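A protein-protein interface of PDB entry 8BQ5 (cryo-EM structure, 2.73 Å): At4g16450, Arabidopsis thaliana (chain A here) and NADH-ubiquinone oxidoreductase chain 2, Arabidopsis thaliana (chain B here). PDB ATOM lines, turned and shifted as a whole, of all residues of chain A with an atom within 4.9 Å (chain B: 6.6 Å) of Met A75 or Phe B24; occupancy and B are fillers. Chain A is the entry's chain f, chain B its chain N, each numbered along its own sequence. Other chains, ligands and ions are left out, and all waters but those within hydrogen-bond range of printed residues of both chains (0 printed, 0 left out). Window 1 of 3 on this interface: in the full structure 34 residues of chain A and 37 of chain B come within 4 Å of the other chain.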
ATOM      1  N   ILE A  68      23.497 -37.534 -30.691  1.00  0.00           N
ATOM      2  CA  ILE A  68      23.575 -36.597 -29.570  1.00  0.00           C
ATOM      3  C   ILE A  68      24.804 -35.707 -29.714  1.00  0.00           C
ATOM      4  O   ILE A  68      24.745 -34.488 -29.501  1.00  0.00           O
ATOM      5  CB  ILE A  68      23.578 -37.357 -28.232  1.00  0.00           C
ATOM      6  CG1 ILE A  68      22.227 -38.033 -28.000  1.00  0.00           C
ATOM      7  CG2 ILE A  68      23.907 -36.421 -27.078  1.00  0.00           C
ATOM      8  CD1 ILE A  68      22.162 -38.826 -26.721  1.00  0.00           C
ATOM      9  N   LEU A  70      26.517 -34.956 -32.519  1.00  0.00           N
ATOM     10  CA  LEU A  70      26.392 -34.037 -33.677  1.00  0.00           C
ATOM     11  C   LEU A  70      25.539 -32.838 -33.261  1.00  0.00           C
ATOM     12  O   LEU A  70      25.946 -31.711 -33.551  1.00  0.00           O
ATOM     13  CB  LEU A  70      25.744 -34.765 -34.852  1.00  0.00           C
ATOM     14  CG  LEU A  70      26.251 -34.376 -36.238  1.00  0.00           C
ATOM     15  CD1 LEU A  70      27.740 -34.653 -36.361  1.00  0.00           C
ATOM     16  CD2 LEU A  70      25.486 -35.125 -37.318  1.00  0.00           C
ATOM     17  N   MET A  71      24.399 -33.092 -32.615  1.00  0.00           N
ATOM     18  CA  MET A  71      23.545 -32.001 -32.160  1.00  0.00           C
ATOM     19  C   MET A  71      24.295 -31.069 -31.213  1.00  0.00           C
ATOM     20  O   MET A  71      24.326 -29.848 -31.416  1.00  0.00           O
ATOM     21  CB  MET A  71      22.305 -32.572 -31.479  1.00  0.00           C
ATOM     22  CG  MET A  71      21.213 -31.565 -31.220  1.00  0.00           C
ATOM     23  SD  MET A  71      19.678 -32.403 -30.819  1.00  0.00           S
ATOM     24  CE  MET A  71      20.018 -32.823 -29.113  1.00  0.00           C
ATOM     25  N   GLY A  72      24.928 -31.634 -30.181  1.00  0.00           N
ATOM     26  CA  GLY A  72      25.594 -30.806 -29.188  1.00  0.00           C
ATOM     27  C   GLY A  72      26.798 -30.064 -29.738  1.00  0.00           C
ATOM     28  O   GLY A  72      27.040 -28.909 -29.383  1.00  0.00           O
ATOM     29  N   GLY A  73      27.534 -30.737 -30.623  1.00  0.00           N
ATOM     30  CA  GLY A  73      28.720 -30.123 -31.238  1.00  0.00           C
ATOM     31  C   GLY A  73      28.338 -28.986 -32.152  1.00  0.00           C
ATOM     32  O   GLY A  73      29.021 -27.953 -32.096  1.00  0.00           O
ATOM     33  N   PHE A  74      27.305 -29.168 -32.978  1.00  0.00           N
ATOM     34  CA  PHE A  74      26.835 -28.045 -33.823  1.00  0.00           C
ATOM     35  C   PHE A  74      26.384 -26.907 -32.908  1.00  0.00           C
ATOM     36  O   PHE A  74      26.730 -25.756 -33.190  1.00  0.00           O
ATOM     37  CB  PHE A  74      25.705 -28.460 -34.760  1.00  0.00           C
ATOM     38  CG  PHE A  74      25.266 -27.382 -35.713  1.00  0.00           C
ATOM     39  CD1 PHE A  74      26.003 -27.102 -36.852  1.00  0.00           C
ATOM     40  CD2 PHE A  74      24.122 -26.640 -35.469  1.00  0.00           C
ATOM     41  CE1 PHE A  74      25.603 -26.108 -37.727  1.00  0.00           C
ATOM     42  CE2 PHE A  74      23.722 -25.644 -36.346  1.00  0.00           C
ATOM     43  CZ  PHE A  74      24.464 -25.382 -37.473  1.00  0.00           C
ATOM     44  N   MET A  75      25.629 -27.239 -31.856  1.00  0.00           N
ATOM     45  CA  MET A  75      25.149 -26.189 -30.966  1.00  0.00           C
ATOM     46  C   MET A  75      26.306 -25.392 -30.383  1.00  0.00           C
ATOM     47  O   MET A  75      26.264 -24.159 -30.347  1.00  0.00           O
ATOM     48  CB  MET A  75      24.318 -26.803 -29.845  1.00  0.00           C
ATOM     49  CG  MET A  75      22.834 -26.595 -29.976  1.00  0.00           C
ATOM     50  SD  MET A  75      21.958 -27.874 -29.070  1.00  0.00           S
ATOM     51  CE  MET A  75      20.269 -27.397 -29.376  1.00  0.00           C
ATOM     52  N   TYR A  76      27.347 -26.084 -29.923  1.00  0.00           N
ATOM     53  CA  TYR A  76      28.491 -25.409 -29.320  1.00  0.00           C
ATOM     54  C   TYR A  76      29.223 -24.539 -30.336  1.00  0.00           C
ATOM     55  O   TYR A  76      29.595 -23.395 -30.036  1.00  0.00           O
ATOM     56  CB  TYR A  76      29.428 -26.449 -28.710  1.00  0.00           C
ATOM     57  CG  TYR A  76      30.406 -25.880 -27.721  1.00  0.00           C
ATOM     58  CD1 TYR A  76      29.964 -25.280 -26.554  1.00  0.00           C
ATOM     59  CD2 TYR A  76      31.772 -25.948 -27.950  1.00  0.00           C
ATOM     60  CE1 TYR A  76      30.853 -24.759 -25.648  1.00  0.00           C
ATOM     61  CE2 TYR A  76      32.669 -25.428 -27.048  1.00  0.00           C
ATOM     62  CZ  TYR A  76      32.206 -24.835 -25.896  1.00  0.00           C
ATOM     63  OH  TYR A  76      33.098 -24.314 -24.990  1.00  0.00           O
ATOM     64  N   ALA A  77      29.422 -25.056 -31.551  1.00  0.00           N
ATOM     65  CA  ALA A  77      30.092 -24.276 -32.586  1.00  0.00           C
ATOM     66  C   ALA A  77      29.261 -23.067 -33.003  1.00  0.00           C
ATOM     67  O   ALA A  77      29.802 -21.970 -33.186  1.00  0.00           O
ATOM     68  CB  ALA A  77      30.398 -25.158 -33.794  1.00  0.00           C
ATOM     69  N   TYR A  78      27.948 -23.250 -33.179  1.00  0.00           N
ATOM     70  CA  TYR A  78      27.085 -22.128 -33.531  1.00  0.00           C
ATOM     71  C   TYR A  78      27.097 -21.076 -32.438  1.00  0.00           C
ATOM     72  O   TYR A  78      27.152 -19.875 -32.721  1.00  0.00           O
ATOM     73  CB  TYR A  78      25.654 -22.610 -33.784  1.00  0.00           C
ATOM     74  CG  TYR A  78      24.734 -21.526 -34.309  1.00  0.00           C
ATOM     75  CD1 TYR A  78      24.211 -20.554 -33.462  1.00  0.00           C
ATOM     76  CD2 TYR A  78      24.401 -21.466 -35.652  1.00  0.00           C
ATOM     77  CE1 TYR A  78      23.389 -19.561 -33.937  1.00  0.00           C
ATOM     78  CE2 TYR A  78      23.571 -20.476 -36.137  1.00  0.00           C
ATOM     79  CZ  TYR A  78      23.070 -19.526 -35.274  1.00  0.00           C
ATOM     80  OH  TYR A  78      22.244 -18.538 -35.749  1.00  0.00           O
ATOM     81  N   GLN A  79      27.021 -21.512 -31.182  1.00  0.00           N
ATOM     82  CA  GLN A  79      27.142 -20.606 -30.052  1.00  0.00           C
ATOM     83  C   GLN A  79      28.407 -19.771 -30.153  1.00  0.00           C
ATOM     84  O   GLN A  79      28.362 -18.541 -30.064  1.00  0.00           O
ATOM     85  CB  GLN A  79      27.144 -21.424 -28.765  1.00  0.00           C
ATOM     86  CG  GLN A  79      26.465 -20.797 -27.590  1.00  0.00           C
ATOM     87  CD  GLN A  79      26.460 -21.733 -26.408  1.00  0.00           C
ATOM     88  OE1 GLN A  79      25.852 -22.800 -26.453  1.00  0.00           O
ATOM     89  NE2 GLN A  79      27.170 -21.361 -25.359  1.00  0.00           N
ATOM     90  N   LEU B  17      19.317 -18.553 -28.415  1.00  0.00           N
ATOM     91  CA  LEU B  17      20.595 -18.765 -27.748  1.00  0.00           C
ATOM     92  C   LEU B  17      20.445 -18.682 -26.236  1.00  0.00           C
ATOM     93  O   LEU B  17      21.274 -19.223 -25.497  1.00  0.00           O
ATOM     94  CB  LEU B  17      21.618 -17.740 -28.234  1.00  0.00           C
ATOM     95  CG  LEU B  17      22.194 -17.950 -29.634  1.00  0.00           C
ATOM     96  CD1 LEU B  17      22.996 -16.731 -30.062  1.00  0.00           C
ATOM     97  CD2 LEU B  17      23.040 -19.210 -29.693  1.00  0.00           C
ATOM     98  N   VAL B  19      18.227 -20.218 -24.635  1.00  0.00           N
ATOM     99  CA  VAL B  19      17.724 -21.508 -24.171  1.00  0.00           C
ATOM    100  C   VAL B  19      18.384 -22.673 -24.901  1.00  0.00           C
ATOM    101  O   VAL B  19      17.779 -23.739 -25.044  1.00  0.00           O
ATOM    102  CB  VAL B  19      16.191 -21.589 -24.309  1.00  0.00           C
ATOM    103  CG1 VAL B  19      15.514 -20.830 -23.180  1.00  0.00           C
ATOM    104  CG2 VAL B  19      15.737 -21.061 -25.661  1.00  0.00           C
ATOM    105  N   PHE B  20      19.622 -22.490 -25.368  1.00  0.00           N
ATOM    106  CA  PHE B  20      20.361 -23.615 -25.943  1.00  0.00           C
ATOM    107  C   PHE B  20      20.541 -24.788 -24.985  1.00  0.00           C
ATOM    108  O   PHE B  20      20.331 -25.936 -25.413  1.00  0.00           O
ATOM    109  CB  PHE B  20      21.716 -23.138 -26.485  1.00  0.00           C
ATOM    110  CG  PHE B  20      21.737 -22.925 -27.973  1.00  0.00           C
ATOM    111  CD1 PHE B  20      20.618 -22.474 -28.645  1.00  0.00           C
ATOM    112  CD2 PHE B  20      22.881 -23.207 -28.704  1.00  0.00           C
ATOM    113  CE1 PHE B  20      20.642 -22.289 -30.012  1.00  0.00           C
ATOM    114  CE2 PHE B  20      22.911 -23.025 -30.070  1.00  0.00           C
ATOM    115  CZ  PHE B  20      21.789 -22.568 -30.726  1.00  0.00           C
ATOM    116  N   PRO B  21      20.948 -24.602 -23.719  1.00  0.00           N
ATOM    117  CA  PRO B  21      21.110 -25.776 -22.840  1.00  0.00           C
ATOM    118  C   PRO B  21      19.835 -26.584 -22.661  1.00  0.00           C
ATOM    119  O   PRO B  21      19.862 -27.820 -22.759  1.00  0.00           O
ATOM    120  CB  PRO B  21      21.580 -25.150 -21.520  1.00  0.00           C
ATOM    121  CG  PRO B  21      22.217 -23.876 -21.914  1.00  0.00           C
ATOM    122  CD  PRO B  21      21.387 -23.365 -23.047  1.00  0.00           C
ATOM    123  N   GLU B  22      18.709 -25.912 -22.408  1.00  0.00           N
ATOM    124  CA  GLU B  22      17.451 -26.625 -22.211  1.00  0.00           C
ATOM    125  C   GLU B  22      16.990 -27.300 -23.497  1.00  0.00           C
ATOM    126  O   GLU B  22      16.522 -28.444 -23.464  1.00  0.00           O
ATOM    127  CB  GLU B  22      16.372 -25.678 -21.673  1.00  0.00           C
ATOM    128  CG  GLU B  22      16.579 -25.070 -20.265  1.00  0.00           C
ATOM    129  CD  GLU B  22      17.427 -23.811 -20.233  1.00  0.00           C
ATOM    130  OE1 GLU B  22      17.918 -23.414 -21.288  1.00  0.00           O
ATOM    131  OE2 GLU B  22      17.615 -23.226 -19.148  1.00  0.00           O
ATOM    132  N   ILE B  23      17.123 -26.621 -24.638  1.00  0.00           N
ATOM    133  CA  ILE B  23      16.759 -27.240 -25.911  1.00  0.00           C
ATOM    134  C   ILE B  23      17.576 -28.506 -26.129  1.00  0.00           C
ATOM    135  O   ILE B  23      17.034 -29.566 -26.477  1.00  0.00           O
ATOM    136  CB  ILE B  23      16.938 -26.244 -27.073  1.00  0.00           C
ATOM    137  CG1 ILE B  23      15.859 -25.162 -27.026  1.00  0.00           C
ATOM    138  CG2 ILE B  23      16.880 -26.963 -28.412  1.00  0.00           C
ATOM    139  CD1 ILE B  23      16.043 -24.081 -28.065  1.00  0.00           C
ATOM    140  N   PHE B  24      18.888 -28.424 -25.895  1.00  0.00           N
ATOM    141  CA  PHE B  24      19.736 -29.590 -26.108  1.00  0.00           C
ATOM    142  C   PHE B  24      19.347 -30.734 -25.184  1.00  0.00           C
ATOM    143  O   PHE B  24      19.234 -31.883 -25.624  1.00  0.00           O
ATOM    144  CB  PHE B  24      21.212 -29.253 -25.906  1.00  0.00           C
ATOM    145  CG  PHE B  24      22.081 -30.474 -25.855  1.00  0.00           C
ATOM    146  CD1 PHE B  24      22.401 -31.153 -27.017  1.00  0.00           C
ATOM    147  CD2 PHE B  24      22.521 -30.983 -24.645  1.00  0.00           C
ATOM    148  CE1 PHE B  24      23.173 -32.294 -26.978  1.00  0.00           C
ATOM    149  CE2 PHE B  24      23.291 -32.127 -24.601  1.00  0.00           C
ATOM    150  CZ  PHE B  24      23.615 -32.782 -25.769  1.00  0.00           C
ATOM    151  N   ILE B  25      19.167 -30.452 -23.891  1.00  0.00           N
ATOM    152  CA  ILE B  25      18.934 -31.545 -22.951  1.00  0.00           C
ATOM    153  C   ILE B  25      17.568 -32.182 -23.191  1.00  0.00           C
ATOM    154  O   ILE B  25      17.417 -33.405 -23.091  1.00  0.00           O
ATOM    155  CB  ILE B  25      19.116 -31.073 -21.495  1.00  0.00           C
ATOM    156  CG1 ILE B  25      19.069 -32.270 -20.541  1.00  0.00           C
ATOM    157  CG2 ILE B  25      18.078 -30.038 -21.106  1.00  0.00           C
ATOM    158  CD1 ILE B  25      19.798 -32.045 -19.232  1.00  0.00           C
ATOM    159  N   ILE B  26      16.560 -31.378 -23.545  1.00  0.00           N
ATOM    160  CA  ILE B  26      15.243 -31.934 -23.852  1.00  0.00           C
ATOM    161  C   ILE B  26      15.313 -32.816 -25.095  1.00  0.00           C
ATOM    162  O   ILE B  26      14.766 -33.928 -25.124  1.00  0.00           O
ATOM    163  CB  ILE B  26      14.210 -30.804 -24.012  1.00  0.00           C
ATOM    164  CG1 ILE B  26      13.964 -30.111 -22.669  1.00  0.00           C
ATOM    165  CG2 ILE B  26      12.911 -31.337 -24.586  1.00  0.00           C
ATOM    166  CD1 ILE B  26      13.348 -28.731 -22.795  1.00  0.00           C
ATOM    167  N   ASN B  27      15.997 -32.340 -26.141  1.00  0.00           N
ATOM    168  CA  ASN B  27      16.104 -33.136 -27.360  1.00  0.00           C
ATOM    169  C   ASN B  27      16.884 -34.425 -27.115  1.00  0.00           C
ATOM    170  O   ASN B  27      16.526 -35.488 -27.640  1.00  0.00           O
ATOM    171  CB  ASN B  27      16.758 -32.308 -28.462  1.00  0.00           C
ATOM    172  CG  ASN B  27      15.856 -31.216 -28.987  1.00  0.00           C
ATOM    173  OD1 ASN B  27      14.636 -31.284 -28.861  1.00  0.00           O
ATOM    174  ND2 ASN B  27      16.459 -30.193 -29.584  1.00  0.00           N
ATOM    175  N   ALA B  28      17.956 -34.351 -26.323  1.00  0.00           N
ATOM    176  CA  ALA B  28      18.728 -35.544 -25.992  1.00  0.00           C
ATOM    177  C   ALA B  28      17.892 -36.537 -25.199  1.00  0.00           C
ATOM    178  O   ALA B  28      17.998 -37.752 -25.400  1.00  0.00           O
ATOM    179  CB  ALA B  28      19.985 -35.157 -25.214  1.00  0.00           C
ATOM    180  N   THR B  29      17.062 -36.040 -24.281  1.00  0.00           N
ATOM    181  CA  THR B  29      16.170 -36.918 -23.536  1.00  0.00           C
ATOM    182  C   THR B  29      15.181 -37.611 -24.465  1.00  0.00           C
ATOM    183  O   THR B  29      14.886 -38.799 -24.297  1.00  0.00           O
ATOM    184  CB  THR B  29      15.438 -36.120 -22.458  1.00  0.00           C
ATOM    185  OG1 THR B  29      16.399 -35.508 -21.589  1.00  0.00           O
ATOM    186  CG2 THR B  29      14.533 -37.019 -21.642  1.00  0.00           C
ATOM    187  N   LEU B  60      26.545 -38.349 -20.533  1.00  0.00           N
ATOM    188  CA  LEU B  60      27.148 -37.563 -21.606  1.00  0.00           C
ATOM    189  C   LEU B  60      26.289 -36.350 -21.954  1.00  0.00           C
ATOM    190  O   LEU B  60      26.811 -35.242 -22.138  1.00  0.00           O
ATOM    191  CB  LEU B  60      27.359 -38.448 -22.833  1.00  0.00           C
ATOM    192  CG  LEU B  60      27.766 -37.784 -24.148  1.00  0.00           C
ATOM    193  CD1 LEU B  60      29.268 -37.547 -24.198  1.00  0.00           C
ATOM    194  CD2 LEU B  60      27.305 -38.629 -25.325  1.00  0.00           C
ATOM    195  N   SER B  61      24.970 -36.541 -22.049  1.00  0.00           N
ATOM    196  CA  SER B  61      24.077 -35.431 -22.377  1.00  0.00           C
ATOM    197  C   SER B  61      24.118 -34.349 -21.304  1.00  0.00           C
ATOM    198  O   SER B  61      24.127 -33.152 -21.616  1.00  0.00           O
ATOM    199  CB  SER B  61      22.648 -35.942 -22.563  1.00  0.00           C
ATOM    200  OG  SER B  61      22.610 -37.057 -23.433  1.00  0.00           O
ATOM    201  N   VAL B  62      24.136 -34.751 -20.032  1.00  0.00           N
ATOM    202  CA  VAL B  62      24.212 -33.789 -18.937  1.00  0.00           C
ATOM    203  C   VAL B  62      25.518 -33.009 -19.007  1.00  0.00           C
ATOM    204  O   VAL B  62      25.539 -31.787 -18.817  1.00  0.00           O
ATOM    205  CB  VAL B  62      24.045 -34.507 -17.584  1.00  0.00           C
ATOM    206  CG1 VAL B  62      24.390 -33.574 -16.435  1.00  0.00           C
ATOM    207  CG2 VAL B  62      22.628 -35.032 -17.428  1.00  0.00           C
ATOM    208  N   LEU B  63      26.627 -33.700 -19.284  1.00  0.00           N
ATOM    209  CA  LEU B  63      27.914 -33.015 -19.375  1.00  0.00           C
ATOM    210  C   LEU B  63      27.950 -32.037 -20.547  1.00  0.00           C
ATOM    211  O   LEU B  63      28.515 -30.942 -20.432  1.00  0.00           O
ATOM    212  CB  LEU B  63      29.045 -34.037 -19.482  1.00  0.00           C
ATOM    213  CG  LEU B  63      29.257 -34.882 -18.224  1.00  0.00           C
ATOM    214  CD1 LEU B  63      30.386 -35.882 -18.410  1.00  0.00           C
ATOM    215  CD2 LEU B  63      29.514 -33.993 -17.020  1.00  0.00           C
ATOM    216  N   ILE B  64      27.354 -32.409 -21.682  1.00  0.00           N
ATOM    217  CA  ILE B  64      27.326 -31.504 -22.827  1.00  0.00           C
ATOM    218  C   ILE B  64      26.440 -30.298 -22.534  1.00  0.00           C
ATOM    219  O   ILE B  64      26.750 -29.169 -22.935  1.00  0.00           O
ATOM    220  CB  ILE B  64      26.875 -32.253 -24.095  1.00  0.00           C
ATOM    221  CG1 ILE B  64      27.937 -33.263 -24.518  1.00  0.00           C
ATOM    222  CG2 ILE B  64      26.645 -31.279 -25.240  1.00  0.00           C
ATOM    223  CD1 ILE B  64      27.484 -34.195 -25.614  1.00  0.00           C
ATOM    224  N   THR B  65      25.327 -30.512 -21.826  1.00  0.00           N
ATOM    225  CA  THR B  65      24.501 -29.388 -21.394  1.00  0.00           C
ATOM    226  C   THR B  65      25.283 -28.459 -20.477  1.00  0.00           C
ATOM    227  O   THR B  65      25.173 -27.232 -20.580  1.00  0.00           O
ATOM    228  CB  THR B  65      23.244 -29.894 -20.684  1.00  0.00           C
ATOM    229  OG1 THR B  65      22.705 -31.014 -21.396  1.00  0.00           O
ATOM    230  CG2 THR B  65      22.198 -28.793 -20.602  1.00  0.00           C
ATOM    231  N   LEU B  66      26.070 -29.031 -19.565  1.00  0.00           N
ATOM    232  CA  LEU B  66      26.877 -28.210 -18.671  1.00  0.00           C
ATOM    233  C   LEU B  66      27.908 -27.404 -19.449  1.00  0.00           C
ATOM    234  O   LEU B  66      28.147 -26.233 -19.140  1.00  0.00           O
ATOM    235  CB  LEU B  66      27.551 -29.086 -17.616  1.00  0.00           C
ATOM    236  CG  LEU B  66      28.585 -28.397 -16.727  1.00  0.00           C
ATOM    237  CD1 LEU B  66      27.948 -27.255 -15.965  1.00  0.00           C
ATOM    238  CD2 LEU B  66      29.186 -29.394 -15.764  1.00  0.00           C
ATOM    239  N   LEU B  68      27.603 -26.403 -22.599  1.00  0.00           N
ATOM    240  CA  LEU B  68      26.870 -25.379 -23.339  1.00  0.00           C
ATOM    241  C   LEU B  68      26.466 -24.226 -22.431  1.00  0.00           C
ATOM    242  O   LEU B  68      26.507 -23.060 -22.838  1.00  0.00           O
ATOM    243  CB  LEU B  68      25.633 -25.988 -23.999  1.00  0.00           C
ATOM    244  CG  LEU B  68      25.819 -26.813 -25.272  1.00  0.00           C
ATOM    245  CD1 LEU B  68      24.517 -27.499 -25.659  1.00  0.00           C
ATOM    246  CD2 LEU B  68      26.313 -25.943 -26.407  1.00  0.00           C
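The backbone carbonyl oxygen (O) of Leu B68 is in hydrogen-bond range of the side-chain amide nitrogen (NE2) of Gln A79 (3.1 Å).
ND2 of Asn B27 sits at hydrogen-bond distance from O of Ile B23, at 3.2 Å.
The side-chain hydroxyl (OG1) of Thr B65 sits at hydrogen-bond distance from the backbone carbonyl oxygen (O) of Ser B61.
Ile A68 touches Phe B24.
Ile A68 touches Ser B61 (CD1 to OG, 3.8 Å).
Met A71 touches Phe B24 (CE to CD1, 3.6 Å).
CB of Asn B27 touches CE of Met A71 (3.4 Å).
CE of Met A71 touches N of Ala B28, at 3.8 Å.
Gly A72 touches Phe B24.
Phe B20 touches Met A75.
Met A75 touches Phe B24.
Leu B68 touches Tyr A76 (CD2 to N, 3.7 Å).
OE1 of Gln A79 touches CD2 of Phe B20 (3.7 Å).
Of the printed residues of chain B, Met A75 touches Phe B20, Ile B23 and Phe B24.
Phe B24 touches just these residues of chain A: Ile A68 (3.7 Å), Met A71 (3.6 Å), Gly A72 (3.6 Å) and Met A75 (3.5 Å).
Of the printed residues of chain A, Asn B27 touches Met A71.
Of the printed residues of chain A, Ala B28 touches Met A71 (3.8 Å).
Of the printed residues of chain A, Leu B68 touches Tyr A76 and Gln A79.
Among the printed residues, 12 pairs touch across the chains.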
